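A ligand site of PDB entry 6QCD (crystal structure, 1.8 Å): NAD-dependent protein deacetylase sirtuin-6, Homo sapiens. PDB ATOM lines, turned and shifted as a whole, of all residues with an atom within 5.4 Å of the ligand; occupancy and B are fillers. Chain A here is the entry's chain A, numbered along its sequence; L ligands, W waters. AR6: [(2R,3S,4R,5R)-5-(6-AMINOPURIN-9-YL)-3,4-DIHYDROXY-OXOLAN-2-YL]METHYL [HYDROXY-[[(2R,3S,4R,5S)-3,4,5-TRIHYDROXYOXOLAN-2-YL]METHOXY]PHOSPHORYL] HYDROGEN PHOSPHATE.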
ATOM      1  N   GLU A  16      -6.669  20.902 -30.730  1.00  0.00           N
ATOM      2  CA  GLU A  16      -8.116  20.674 -30.863  1.00  0.00           C
ATOM      3  C   GLU A  16      -8.540  21.163 -32.240  1.00  0.00           C
ATOM      4  O   GLU A  16      -7.943  22.149 -32.740  1.00  0.00           O
ATOM      5  CB  GLU A  16      -8.866  21.443 -29.799  1.00  0.00           C
ATOM      6  CG  GLU A  16      -8.645  20.949 -28.402  1.00  0.00           C
ATOM      7  CD  GLU A  16      -9.404  21.634 -27.293  1.00  0.00           C
ATOM      8  OE1 GLU A  16      -9.600  22.853 -27.369  1.00  0.00           O
ATOM      9  OE2 GLU A  16      -9.780  20.923 -26.322  1.00  0.00           O
ATOM     10  N   THR A  45     -17.497   5.492 -24.812  1.00  0.00           N
ATOM     11  CA  THR A  45     -17.171   6.771 -24.145  1.00  0.00           C
ATOM     12  C   THR A  45     -15.813   6.742 -23.457  1.00  0.00           C
ATOM     13  O   THR A  45     -15.376   5.731 -22.823  1.00  0.00           O
ATOM     14  CB  THR A  45     -18.288   7.190 -23.168  1.00  0.00           C
ATOM     15  OG1 THR A  45     -18.427   6.261 -22.122  1.00  0.00           O
ATOM     16  CG2 THR A  45     -19.621   7.347 -23.848  1.00  0.00           C
ATOM     17  N   GLY A  46     -15.235   7.935 -23.395  1.00  0.00           N
ATOM     18  CA  GLY A  46     -14.019   8.206 -22.636  1.00  0.00           C
ATOM     19  C   GLY A  46     -14.170   9.471 -21.836  1.00  0.00           C
ATOM     20  O   GLY A  46     -15.313  10.022 -21.759  1.00  0.00           O
ATOM     21  N   ALA A  47     -13.036   9.955 -21.358  1.00  0.00           N
ATOM     22  CA  ALA A  47     -12.967  11.028 -20.333  1.00  0.00           C
ATOM     23  C   ALA A  47     -13.486  12.359 -20.882  1.00  0.00           C
ATOM     24  O   ALA A  47     -14.006  13.195 -20.049  1.00  0.00           O
ATOM     25  CB  ALA A  47     -11.554  11.162 -19.809  1.00  0.00           C
ATOM     26  N   GLY A  48     -13.538  12.532 -22.187  1.00  0.00           N
ATOM     27  CA  GLY A  48     -14.093  13.751 -22.828  1.00  0.00           C
ATOM     28  C   GLY A  48     -15.560  13.995 -22.470  1.00  0.00           C
ATOM     29  O   GLY A  48     -16.006  15.120 -22.540  1.00  0.00           O
ATOM     30  N   ILE A  49     -16.348  12.965 -22.189  1.00  0.00           N
ATOM     31  CA  ILE A  49     -17.782  13.205 -21.874  1.00  0.00           C
ATOM     32  C   ILE A  49     -17.968  13.740 -20.452  1.00  0.00           C
ATOM     33  O   ILE A  49     -19.115  13.946 -20.047  1.00  0.00           O
ATOM     34  CB  ILE A  49     -18.620  11.937 -22.122  1.00  0.00           C
ATOM     35  CG1 ILE A  49     -18.494  10.833 -21.078  1.00  0.00           C
ATOM     36  CG2 ILE A  49     -18.464  11.406 -23.545  1.00  0.00           C
ATOM     37  CD1 ILE A  49     -19.808  10.024 -21.057  1.00  0.00           C
ATOM     38  N   THR A  51     -15.608  16.093 -18.870  1.00  0.00           N
ATOM     39  CA  THR A  51     -14.902  17.381 -18.746  1.00  0.00           C
ATOM     40  C   THR A  51     -15.896  18.496 -18.432  1.00  0.00           C
ATOM     41  O   THR A  51     -15.582  19.344 -17.581  1.00  0.00           O
ATOM     42  CB  THR A  51     -14.032  17.687 -19.973  1.00  0.00           C
ATOM     43  OG1 THR A  51     -14.824  17.709 -21.143  1.00  0.00           O
ATOM     44  CG2 THR A  51     -12.836  16.763 -20.112  1.00  0.00           C
ATOM     45  N   ALA A  52     -17.106  18.452 -18.987  1.00  0.00           N
ATOM     46  CA  ALA A  52     -18.117  19.495 -18.741  1.00  0.00           C
ATOM     47  C   ALA A  52     -18.793  19.324 -17.374  1.00  0.00           C
ATOM     48  O   ALA A  52     -19.555  20.249 -17.074  1.00  0.00           O
ATOM     49  CB  ALA A  52     -19.156  19.489 -19.825  1.00  0.00           C
ATOM     50  N   ASP A  57      -9.827  15.458 -18.437  1.00  0.00           N
ATOM     51  CA  ASP A  57      -9.518  14.215 -19.189  1.00  0.00           C
ATOM     52  C   ASP A  57      -8.032  13.850 -18.936  1.00  0.00           C
ATOM     53  O   ASP A  57      -7.418  14.455 -18.028  1.00  0.00           O
ATOM     54  CB  ASP A  57      -9.991  14.428 -20.638  1.00  0.00           C
ATOM     55  CG  ASP A  57      -9.245  15.535 -21.403  1.00  0.00           C
ATOM     56  OD1 ASP A  57      -8.163  15.942 -21.002  1.00  0.00           O
ATOM     57  OD2 ASP A  57      -9.786  15.990 -22.407  1.00  0.00           O
ATOM     58  N   PHE A  58      -7.484  12.924 -19.716  1.00  0.00           N
ATOM     59  CA  PHE A  58      -6.055  12.497 -19.617  1.00  0.00           C
ATOM     60  C   PHE A  58      -5.166  13.191 -20.645  1.00  0.00           C
ATOM     61  O   PHE A  58      -4.035  13.536 -20.250  1.00  0.00           O
ATOM     62  CB  PHE A  58      -5.979  10.979 -19.766  1.00  0.00           C
ATOM     63  CG  PHE A  58      -6.673  10.309 -18.616  1.00  0.00           C
ATOM     64  CD1 PHE A  58      -5.960  10.065 -17.463  1.00  0.00           C
ATOM     65  CD2 PHE A  58      -8.030   9.985 -18.659  1.00  0.00           C
ATOM     66  CE1 PHE A  58      -6.585   9.541 -16.342  1.00  0.00           C
ATOM     67  CE2 PHE A  58      -8.623   9.407 -17.543  1.00  0.00           C
ATOM     68  CZ  PHE A  58      -7.895   9.197 -16.388  1.00  0.00           C
ATOM     69  N   ARG A  59      -5.625  13.435 -21.891  1.00  0.00           N
ATOM     70  CA  ARG A  59      -4.711  13.725 -23.011  1.00  0.00           C
ATOM     71  C   ARG A  59      -5.150  14.999 -23.700  1.00  0.00           C
ATOM     72  O   ARG A  59      -4.486  15.373 -24.672  1.00  0.00           O
ATOM     73  CB  ARG A  59      -4.582  12.515 -23.936  1.00  0.00           C
ATOM     74  CG  ARG A  59      -4.019  11.303 -23.221  1.00  0.00           C
ATOM     75  CD  ARG A  59      -3.757  10.151 -24.143  1.00  0.00           C
ATOM     76  NE  ARG A  59      -3.331   8.997 -23.397  1.00  0.00           N
ATOM     77  CZ  ARG A  59      -4.141   8.187 -22.712  1.00  0.00           C
ATOM     78  NH1 ARG A  59      -5.462   8.371 -22.703  1.00  0.00           N
ATOM     79  NH2 ARG A  59      -3.595   7.165 -22.070  1.00  0.00           N
ATOM     80  N   GLY A  60      -6.228  15.655 -23.233  1.00  0.00           N
ATOM     81  CA  GLY A  60      -6.645  16.988 -23.698  1.00  0.00           C
ATOM     82  C   GLY A  60      -5.594  18.061 -23.408  1.00  0.00           C
ATOM     83  O   GLY A  60      -4.572  17.777 -22.775  1.00  0.00           O
ATOM     84  N   PRO A  61      -5.801  19.332 -23.821  1.00  0.00           N
ATOM     85  CA  PRO A  61      -4.797  20.384 -23.529  1.00  0.00           C
ATOM     86  C   PRO A  61      -4.467  20.570 -22.030  1.00  0.00           C
ATOM     87  O   PRO A  61      -3.321  20.930 -21.689  1.00  0.00           O
ATOM     88  CB  PRO A  61      -5.402  21.677 -24.083  1.00  0.00           C
ATOM     89  CG  PRO A  61      -6.450  21.194 -25.095  1.00  0.00           C
ATOM     90  CD  PRO A  61      -6.904  19.816 -24.628  1.00  0.00           C
ATOM     91  N   TRP A  65      -2.368  13.646 -17.871  1.00  0.00           N
ATOM     92  CA  TRP A  65      -1.055  13.241 -18.446  1.00  0.00           C
ATOM     93  C   TRP A  65      -0.405  14.425 -19.175  1.00  0.00           C
ATOM     94  O   TRP A  65       0.807  14.637 -18.952  1.00  0.00           O
ATOM     95  CB  TRP A  65      -1.158  12.033 -19.365  1.00  0.00           C
ATOM     96  CG  TRP A  65      -1.772  10.788 -18.844  1.00  0.00           C
ATOM     97  CD1 TRP A  65      -2.371   9.872 -19.656  1.00  0.00           C
ATOM     98  CD2 TRP A  65      -1.800  10.228 -17.522  1.00  0.00           C
ATOM     99  NE1 TRP A  65      -2.825   8.804 -18.937  1.00  0.00           N
ATOM    100  CE2 TRP A  65      -2.491   8.999 -17.618  1.00  0.00           C
ATOM    101  CE3 TRP A  65      -1.318  10.623 -16.260  1.00  0.00           C
ATOM    102  CZ2 TRP A  65      -2.700   8.161 -16.532  1.00  0.00           C
ATOM    103  CZ3 TRP A  65      -1.538   9.805 -15.178  1.00  0.00           C
ATOM    104  CH2 TRP A  65      -2.238   8.602 -15.304  1.00  0.00           C
ATOM    105  N   GLN A 107     -14.521   3.611 -20.991  1.00  0.00           N
ATOM    106  CA  GLN A 107     -13.203   3.540 -20.336  1.00  0.00           C
ATOM    107  C   GLN A 107     -13.187   4.320 -19.031  1.00  0.00           C
ATOM    108  O   GLN A 107     -12.128   4.389 -18.447  1.00  0.00           O
ATOM    109  CB  GLN A 107     -12.180   4.064 -21.369  1.00  0.00           C
ATOM    110  CG  GLN A 107     -12.041   3.151 -22.589  1.00  0.00           C
ATOM    111  CD  GLN A 107     -11.232   3.800 -23.682  1.00  0.00           C
ATOM    112  OE1 GLN A 107     -10.022   3.924 -23.581  1.00  0.00           O
ATOM    113  NE2 GLN A 107     -11.888   4.298 -24.702  1.00  0.00           N
ATOM    114  N   ASN A 108     -14.281   4.980 -18.644  1.00  0.00           N
ATOM    115  CA  ASN A 108     -14.305   5.993 -17.578  1.00  0.00           C
ATOM    116  C   ASN A 108     -14.420   5.247 -16.251  1.00  0.00           C
ATOM    117  O   ASN A 108     -15.246   4.273 -16.162  1.00  0.00           O
ATOM    118  CB  ASN A 108     -15.419   7.034 -17.750  1.00  0.00           C
ATOM    119  CG  ASN A 108     -15.184   7.905 -18.965  1.00  0.00           C
ATOM    120  OD1 ASN A 108     -14.050   7.984 -19.443  1.00  0.00           O
ATOM    121  ND2 ASN A 108     -16.247   8.507 -19.468  1.00  0.00           N
ATOM    122  N   HIS A 127     -12.246  -0.170 -17.456  1.00  0.00           N
ATOM    123  CA  HIS A 127     -11.070   0.261 -16.654  1.00  0.00           C
ATOM    124  C   HIS A 127     -11.454   0.291 -15.166  1.00  0.00           C
ATOM    125  O   HIS A 127     -10.605   0.697 -14.367  1.00  0.00           O
ATOM    126  CB  HIS A 127     -10.473   1.596 -17.169  1.00  0.00           C
ATOM    127  CG  HIS A 127     -10.008   1.528 -18.598  1.00  0.00           C
ATOM    128  ND1 HIS A 127      -9.588   2.635 -19.338  1.00  0.00           N
ATOM    129  CD2 HIS A 127      -9.942   0.462 -19.434  1.00  0.00           C
ATOM    130  CE1 HIS A 127      -9.294   2.248 -20.570  1.00  0.00           C
ATOM    131  NE2 HIS A 127      -9.488   0.898 -20.647  1.00  0.00           N
ATOM    132  N   TRP A 182      -1.709  -0.183 -14.494  1.00  0.00           N
ATOM    133  CA  TRP A 182      -1.070  -0.286 -15.838  1.00  0.00           C
ATOM    134  C   TRP A 182      -0.863  -1.762 -16.197  1.00  0.00           C
ATOM    135  O   TRP A 182      -1.203  -2.128 -17.316  1.00  0.00           O
ATOM    136  CB  TRP A 182       0.262   0.507 -15.862  1.00  0.00           C
ATOM    137  CG  TRP A 182       0.067   1.989 -15.849  1.00  0.00           C
ATOM    138  CD1 TRP A 182       0.270   2.845 -14.804  1.00  0.00           C
ATOM    139  CD2 TRP A 182      -0.406   2.812 -16.941  1.00  0.00           C
ATOM    140  NE1 TRP A 182      -0.040   4.135 -15.166  1.00  0.00           N
ATOM    141  CE2 TRP A 182      -0.457   4.140 -16.472  1.00  0.00           C
ATOM    142  CE3 TRP A 182      -0.813   2.538 -18.252  1.00  0.00           C
ATOM    143  CZ2 TRP A 182      -0.859   5.200 -17.296  1.00  0.00           C
ATOM    144  CZ3 TRP A 182      -1.214   3.586 -19.065  1.00  0.00           C
ATOM    145  CH2 TRP A 182      -1.247   4.894 -18.585  1.00  0.00           C
ATOM    146  N   GLY A 208     -15.713  11.522 -26.924  1.00  0.00           N
ATOM    147  CA  GLY A 208     -14.694  12.036 -25.979  1.00  0.00           C
ATOM    148  C   GLY A 208     -13.714  10.959 -25.580  1.00  0.00           C
ATOM    149  O   GLY A 208     -13.357  10.865 -24.399  1.00  0.00           O
ATOM    150  N   THR A 209     -13.319  10.112 -26.529  1.00  0.00           N
ATOM    151  CA  THR A 209     -12.116   9.264 -26.390  1.00  0.00           C
ATOM    152  C   THR A 209     -11.104   9.437 -27.548  1.00  0.00           C
ATOM    153  O   THR A 209     -11.477   9.490 -28.703  1.00  0.00           O
ATOM    154  CB  THR A 209     -12.492   7.801 -26.172  1.00  0.00           C
ATOM    155  OG1 THR A 209     -11.276   7.110 -26.025  1.00  0.00           O
ATOM    156  CG2 THR A 209     -13.263   7.205 -27.316  1.00  0.00           C
ATOM    157  N   SER A 210      -9.804   9.440 -27.195  1.00  0.00           N
ATOM    158  CA  SER A 210      -8.702   9.590 -28.166  1.00  0.00           C
ATOM    159  C   SER A 210      -8.352   8.213 -28.745  1.00  0.00           C
ATOM    160  O   SER A 210      -7.632   8.144 -29.743  1.00  0.00           O
ATOM    161  CB  SER A 210      -7.517  10.357 -27.549  1.00  0.00           C
ATOM    162  OG  SER A 210      -6.885   9.581 -26.571  1.00  0.00           O
ATOM    163  N   LEU A 211      -8.890   7.145 -28.152  1.00  0.00           N
ATOM    164  CA  LEU A 211      -8.856   5.751 -28.716  1.00  0.00           C
ATOM    165  C   LEU A 211      -7.406   5.204 -28.760  1.00  0.00           C
ATOM    166  O   LEU A 211      -7.112   4.313 -29.607  1.00  0.00           O
ATOM    167  CB  LEU A 211      -9.493   5.698 -30.109  1.00  0.00           C
ATOM    168  CG  LEU A 211     -10.993   6.010 -30.230  1.00  0.00           C
ATOM    169  CD1 LEU A 211     -11.424   6.031 -31.670  1.00  0.00           C
ATOM    170  CD2 LEU A 211     -11.846   5.030 -29.432  1.00  0.00           C
ATOM    171  N   GLN A 212      -6.561   5.658 -27.849  1.00  0.00           N
ATOM    172  CA  GLN A 212      -5.128   5.320 -27.817  1.00  0.00           C
ATOM    173  C   GLN A 212      -4.908   4.045 -26.997  1.00  0.00           C
ATOM    174  O   GLN A 212      -3.849   3.475 -27.162  1.00  0.00           O
ATOM    175  CB  GLN A 212      -4.364   6.502 -27.250  1.00  0.00           C
ATOM    176  CG  GLN A 212      -4.464   7.741 -28.124  1.00  0.00           C
ATOM    177  CD  GLN A 212      -3.420   8.766 -27.721  1.00  0.00           C
ATOM    178  OE1 GLN A 212      -2.254   8.426 -27.597  1.00  0.00           O
ATOM    179  NE2 GLN A 212      -3.831  10.019 -27.536  1.00  0.00           N
ATOM    180  N   ILE A 213      -5.847   3.610 -26.144  1.00  0.00           N
ATOM    181  CA  ILE A 213      -5.616   2.439 -25.264  1.00  0.00           C
ATOM    182  C   ILE A 213      -6.010   1.176 -26.017  1.00  0.00           C
ATOM    183  O   ILE A 213      -7.026   1.147 -26.692  1.00  0.00           O
ATOM    184  CB  ILE A 213      -6.364   2.578 -23.902  1.00  0.00           C
ATOM    185  CG1 ILE A 213      -5.742   3.667 -23.049  1.00  0.00           C
ATOM    186  CG2 ILE A 213      -6.477   1.234 -23.176  1.00  0.00           C
ATOM    187  CD1 ILE A 213      -4.419   3.330 -22.462  1.00  0.00           C
ATOM    188  N   VAL A 233     -16.655  11.148 -32.437  1.00  0.00           N
ATOM    189  CA  VAL A 233     -16.958  12.523 -31.995  1.00  0.00           C
ATOM    190  C   VAL A 233     -15.875  12.898 -30.978  1.00  0.00           C
ATOM    191  O   VAL A 233     -15.708  12.239 -29.968  1.00  0.00           O
ATOM    192  CB  VAL A 233     -18.355  12.660 -31.369  1.00  0.00           C
ATOM    193  CG1 VAL A 233     -18.643  14.086 -30.951  1.00  0.00           C
ATOM    194  CG2 VAL A 233     -19.466  12.068 -32.234  1.00  0.00           C
ATOM    195  N   ASN A 234     -15.078  13.950 -31.253  1.00  0.00           N
ATOM    196  CA  ASN A 234     -13.911  14.280 -30.380  1.00  0.00           C
ATOM    197  C   ASN A 234     -13.282  15.601 -30.803  1.00  0.00           C
ATOM    198  O   ASN A 234     -13.288  15.861 -32.079  1.00  0.00           O
ATOM    199  CB  ASN A 234     -12.803  13.233 -30.471  1.00  0.00           C
ATOM    200  CG  ASN A 234     -11.973  13.127 -29.217  1.00  0.00           C
ATOM    201  OD1 ASN A 234     -12.487  12.767 -28.163  1.00  0.00           O
ATOM    202  ND2 ASN A 234     -10.668  13.295 -29.320  1.00  0.00           N
ATOM    203  N   LEU A 235     -12.774  16.359 -29.834  1.00  0.00           N
ATOM    204  CA  LEU A 235     -12.128  17.685 -30.124  1.00  0.00           C
ATOM    205  C   LEU A 235     -10.710  17.535 -30.717  1.00  0.00           C
ATOM    206  O   LEU A 235     -10.360  18.256 -31.664  1.00  0.00           O
ATOM    207  CB  LEU A 235     -12.131  18.545 -28.868  1.00  0.00           C
ATOM    208  CG  LEU A 235     -13.469  19.148 -28.451  1.00  0.00           C
ATOM    209  CD1 LEU A 235     -13.280  19.801 -27.119  1.00  0.00           C
ATOM    210  CD2 LEU A 235     -14.007  20.131 -29.480  1.00  0.00           C
ATOM    211  N   GLN A 236      -9.985  16.534 -30.288  1.00  0.00           N
ATOM    212  CA  GLN A 236      -8.636  16.229 -30.811  1.00  0.00           C
ATOM    213  C   GLN A 236      -8.742  15.135 -31.870  1.00  0.00           C
ATOM    214  O   GLN A 236      -9.700  14.322 -31.873  1.00  0.00           O
ATOM    215  CB  GLN A 236      -7.782  15.733 -29.659  1.00  0.00           C
ATOM    216  CG  GLN A 236      -7.211  16.827 -28.735  1.00  0.00           C
ATOM    217  CD  GLN A 236      -6.512  16.258 -27.541  1.00  0.00           C
ATOM    218  OE1 GLN A 236      -6.851  15.166 -27.033  1.00  0.00           O
ATOM    219  NE2 GLN A 236      -5.550  17.049 -27.006  1.00  0.00           N
ATOM    220  N   PRO A 237      -7.690  14.993 -32.700  1.00  0.00           N
ATOM    221  CA  PRO A 237      -7.479  13.789 -33.483  1.00  0.00           C
ATOM    222  C   PRO A 237      -7.510  12.575 -32.557  1.00  0.00           C
ATOM    223  O   PRO A 237      -7.190  12.717 -31.388  1.00  0.00           O
ATOM    224  CB  PRO A 237      -6.021  13.913 -34.048  1.00  0.00           C
ATOM    225  CG  PRO A 237      -5.801  15.379 -34.046  1.00  0.00           C
ATOM    226  CD  PRO A 237      -6.534  15.920 -32.830  1.00  0.00           C
ATOM    227  N   GLY A 250     -16.348  18.760 -32.266  1.00  0.00           N
ATOM    228  CA  GLY A 250     -17.122  19.729 -31.470  1.00  0.00           C
ATOM    229  C   GLY A 250     -17.418  19.155 -30.095  1.00  0.00           C
ATOM    230  O   GLY A 250     -16.920  18.024 -29.762  1.00  0.00           O
ATOM    231  N   TYR A 251     -17.917  19.977 -29.228  1.00  0.00           N
ATOM    232  CA  TYR A 251     -18.158  19.556 -27.831  1.00  0.00           C
ATOM    233  C   TYR A 251     -19.234  18.503 -27.856  1.00  0.00           C
ATOM    234  O   TYR A 251     -20.270  18.734 -28.545  1.00  0.00           O
ATOM    235  CB  TYR A 251     -18.573  20.742 -26.971  1.00  0.00           C
ATOM    236  CG  TYR A 251     -17.452  21.714 -26.774  1.00  0.00           C
ATOM    237  CD1 TYR A 251     -16.480  21.511 -25.798  1.00  0.00           C
ATOM    238  CD2 TYR A 251     -17.393  22.864 -27.525  1.00  0.00           C
ATOM    239  CE1 TYR A 251     -15.492  22.450 -25.577  1.00  0.00           C
ATOM    240  CE2 TYR A 251     -16.367  23.783 -27.364  1.00  0.00           C
ATOM    241  CZ  TYR A 251     -15.407  23.568 -26.392  1.00  0.00           C
ATOM    242  OH  TYR A 251     -14.415  24.506 -26.214  1.00  0.00           O
ATOM    243  N   VAL A 252     -19.016  17.421 -27.109  1.00  0.00           N
ATOM    244  CA  VAL A 252     -19.944  16.277 -27.150  1.00  0.00           C
ATOM    245  C   VAL A 252     -21.331  16.689 -26.671  1.00  0.00           C
ATOM    246  O   VAL A 252     -22.275  16.210 -27.279  1.00  0.00           O
ATOM    247  CB  VAL A 252     -19.492  15.050 -26.377  1.00  0.00           C
ATOM    248  CG1 VAL A 252     -18.462  14.317 -27.153  1.00  0.00           C
ATOM    249  CG2 VAL A 252     -19.063  15.342 -24.937  1.00  0.00           C
ATOM    250  N   ASP A 253     -21.452  17.607 -25.695  1.00  0.00           N
ATOM    251  CA  ASP A 253     -22.796  18.077 -25.252  1.00  0.00           C
ATOM    252  C   ASP A 253     -23.528  18.793 -26.384  1.00  0.00           C
ATOM    253  O   ASP A 253     -24.749  18.591 -26.518  1.00  0.00           O
ATOM    254  CB  ASP A 253     -22.740  18.929 -23.995  1.00  0.00           C
ATOM    255  CG  ASP A 253     -22.523  18.128 -22.726  1.00  0.00           C
ATOM    256  OD1 ASP A 253     -22.649  16.849 -22.726  1.00  0.00           O
ATOM    257  OD2 ASP A 253     -22.169  18.775 -21.730  1.00  0.00           O
HETATM  258  N1  AR6 L   1     -16.258  17.341 -26.106  1.00  0.00           N
HETATM  259  C2  AR6 L   1     -15.582  16.628 -27.021  1.00  0.00           C
HETATM  260  N3  AR6 L   1     -14.376  16.052 -26.928  1.00  0.00           N
HETATM  261  C4  AR6 L   1     -13.828  16.274 -25.718  1.00  0.00           C
HETATM  262  C5  AR6 L   1     -14.363  17.035 -24.699  1.00  0.00           C
HETATM  263  C6  AR6 L   1     -15.649  17.592 -24.923  1.00  0.00           C
HETATM  264  N6  AR6 L   1     -16.327  18.320 -24.033  1.00  0.00           N
HETATM  265  N7  AR6 L   1     -13.485  17.095 -23.631  1.00  0.00           N
HETATM  266  C8  AR6 L   1     -12.467  16.330 -23.994  1.00  0.00           C
HETATM  267  N9  AR6 L   1     -12.604  15.830 -25.260  1.00  0.00           N
HETATM  268  PA  AR6 L   1      -8.244  10.902 -23.327  1.00  0.00           P
HETATM  269  PB  AR6 L   1      -9.598   8.347 -22.821  1.00  0.00           P
HETATM  270  C1' AR6 L   1     -11.727  14.945 -25.917  1.00  0.00           C
HETATM  271  O1A AR6 L   1      -7.195  10.133 -24.068  1.00  0.00           O
HETATM  272  O1B AR6 L   1     -10.852   8.152 -22.026  1.00  0.00           O
HETATM  273  C1D AR6 L   1      -6.048   6.655 -19.415  1.00  0.00           C
HETATM  274  O1D AR6 L   1      -4.815   6.103 -19.076  1.00  0.00           O
HETATM  275  C2' AR6 L   1     -10.245  15.314 -25.917  1.00  0.00           C
HETATM  276  O2' AR6 L   1      -9.869  16.117 -27.019  1.00  0.00           O
HETATM  277  O2A AR6 L   1      -8.001  12.059 -22.429  1.00  0.00           O
HETATM  278  O2B AR6 L   1      -9.659   8.090 -24.269  1.00  0.00           O
HETATM  279  C2D AR6 L   1      -7.151   6.058 -18.553  1.00  0.00           C
HETATM  280  O2D AR6 L   1      -6.822   4.744 -18.116  1.00  0.00           O
HETATM  281  C3' AR6 L   1      -9.558  13.952 -25.870  1.00  0.00           C
HETATM  282  O3' AR6 L   1      -8.905  13.557 -27.062  1.00  0.00           O
HETATM  283  O3A AR6 L   1      -9.158   9.874 -22.463  1.00  0.00           O
HETATM  284  C3D AR6 L   1      -8.357   6.182 -19.483  1.00  0.00           C
HETATM  285  O3D AR6 L   1      -9.472   5.399 -19.020  1.00  0.00           O
HETATM  286  C4' AR6 L   1     -10.656  12.944 -25.458  1.00  0.00           C
HETATM  287  O4' AR6 L   1     -11.808  13.736 -25.203  1.00  0.00           O
HETATM  288  C4D AR6 L   1      -7.691   5.733 -20.796  1.00  0.00           C
HETATM  289  O4D AR6 L   1      -6.359   6.301 -20.749  1.00  0.00           O
HETATM  290  C5' AR6 L   1     -10.390  12.132 -24.234  1.00  0.00           C
HETATM  291  O5' AR6 L   1      -9.198  11.335 -24.526  1.00  0.00           O
HETATM  292  C5D AR6 L   1      -8.357   6.199 -22.063  1.00  0.00           C
HETATM  293  O5D AR6 L   1      -8.409   7.645 -22.032  1.00  0.00           O
HETATM  294  O   HOH W   1      -9.653  18.449 -25.933  1.00  0.00           O
HETATM  295  O   HOH W   2     -17.885  17.019 -21.404  1.00  0.00           O
HETATM  296  O   HOH W   3      -7.340   7.152 -25.416  1.00  0.00           O
HETATM  297  O   HOH W   4     -19.374  18.477 -23.766  1.00  0.00           O
HETATM  298  O   HOH W   5      -9.874  18.377 -23.076  1.00  0.00           O
HETATM  299  O   HOH W   6     -11.382   7.266 -19.511  1.00  0.00           O
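The side-chain hydroxyl (OG1) of Thr 209 lies within hydrogen-bond range of the side-chain amide nitrogen (NE2) of Gln 107, 3.2 Å away. N of Leu 211 sits at hydrogen-bond distance from OG1 of Thr 209 (3.2 Å). The side-chain amide nitrogen of Gln 236 lies within hydrogen-bond range of the backbone carbonyl oxygen of Arg 59 (3.1 Å). O of Phe 58 lies within hydrogen-bond range of N of Trp 65 (2.9 Å). N of Gln 107 lies within hydrogen-bond range of O of Thr 45. N of Gly 60 lies within hydrogen-bond range of OD1 of Asp 57. The backbone carbonyl oxygen (O) of Gly 208 sits at hydrogen-bond distance from the backbone NH (N) of Gly 48 (2.8 Å). O of Val 233 sits at hydrogen-bond distance from N of Gly 208, at 3.1 Å.
Water W1 bridges OE2 of Glu 16 (2.5 Å) and O2' of the ligand (2.6 Å). Water W6 lies within hydrogen-bond range of O3D of the ligand (2.7 Å), OD1 of Asn 108 (2.8 Å) and O of Gln 107 (3.2 Å). Water W3 lies within hydrogen-bond range of OG of Ser 210, O2B of the ligand, N of Gln 212 and N of Leu 211. Water W4 bridges N of Asp 253 and N6 of the ligand. Water W2 lies within hydrogen-bond range of the backbone carbonyl oxygen of Gly 48 (2.9 Å), the backbone NH of Ala 52 (2.9 Å), the side-chain hydroxyl of Thr 51 (3.1 Å) and a nitrogen (N6) of the ligand (3.3 Å).
The backbone carbonyl oxygen (O) of Gly 48 lies close to a nitrogen (N7) of the ligand, at 3.4 Å. The backbone carbonyl oxygen (O) of Gly 208 lies close to an oxygen (O4') of the ligand, 3.4 Å away. CA of Gly 46 touches O1B of the ligand, at 3.2 Å. OD2 of Asp 57 touches C8 of the ligand (3.1 Å). Trp 182 touches the ligand (CH2 to O1D, 3.8 Å). Ile 213 touches the ligand (CG1 to O4D, 3.6 Å). O of Gly 250 touches C2 of the ligand, at 3.4 Å. CA of Tyr 251 touches N1 of the ligand, 3.4 Å away. 21 residues have an atom within 4 Å of the ligand: Gly 46, Ala 47, Gly 48, Thr 51, Asp 57, Phe 58, Arg 59, Trp 65, Gln 107, His 127, Trp 182, Gly 208, Thr 209, Ser 210, Ile 213, Asn 234, Leu 235, Gln 236, Gly 250, Tyr 251 and Val 252.
An oxygen (O2B) of the ligand lies within hydrogen-bond range of the side-chain hydroxyl of Thr 209, 2.6 Å away. The backbone NH (N) of Ser 210 lies within hydrogen-bond range of an oxygen (O2B) of the ligand, at 3.2 Å. The side-chain hydroxyl of Ser 210 sits at hydrogen-bond distance from an oxygen (O1A) of the ligand (2.6 Å). An oxygen (O2') of the ligand lies close to the backbone NH (N) of Gln 236 (3.3 Å). An oxygen (O3') of the ligand lies within hydrogen-bond range of the side-chain amide oxygen of Gln 236, 2.6 Å away. O3D of the ligand sits at hydrogen-bond distance from ND1 of His 127 (2.8 Å). An oxygen (O2A) of the ligand is in hydrogen-bond range of the backbone NH (N) of Arg 59 (2.8 Å). An oxygen (O1A) of the ligand is in salt-bridge range of the guanidinium group of Arg 59. An oxygen (O3') of the ligand is in hydrogen-bond range of the side-chain amide nitrogen of Asn 234 (2.9 Å). N7 of the ligand sits at hydrogen-bond distance from OG1 of Thr 51 (2.9 Å). N of Phe 58 lies within hydrogen-bond range of O2A of the ligand (2.9 Å). The backbone carbonyl oxygen (O) of Gln 107 lies within hydrogen-bond range of an oxygen (O3D) of the ligand, at 2.9 Å. The backbone NH (N) of Ala 47 is in hydrogen-bond range of an oxygen (O1B) of the ligand (2.9 Å). The backbone NH (N) of Val 252 is in hydrogen-bond range of a nitrogen (N1) of the ligand, 2.9 Å away. N of Leu 235 is in hydrogen-bond range of N3 of the ligand (3.3 Å). The indole nitrogen of Trp 65 is in hydrogen-bond range of an oxygen (O1D) of the ligand, at 3.4 Å.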
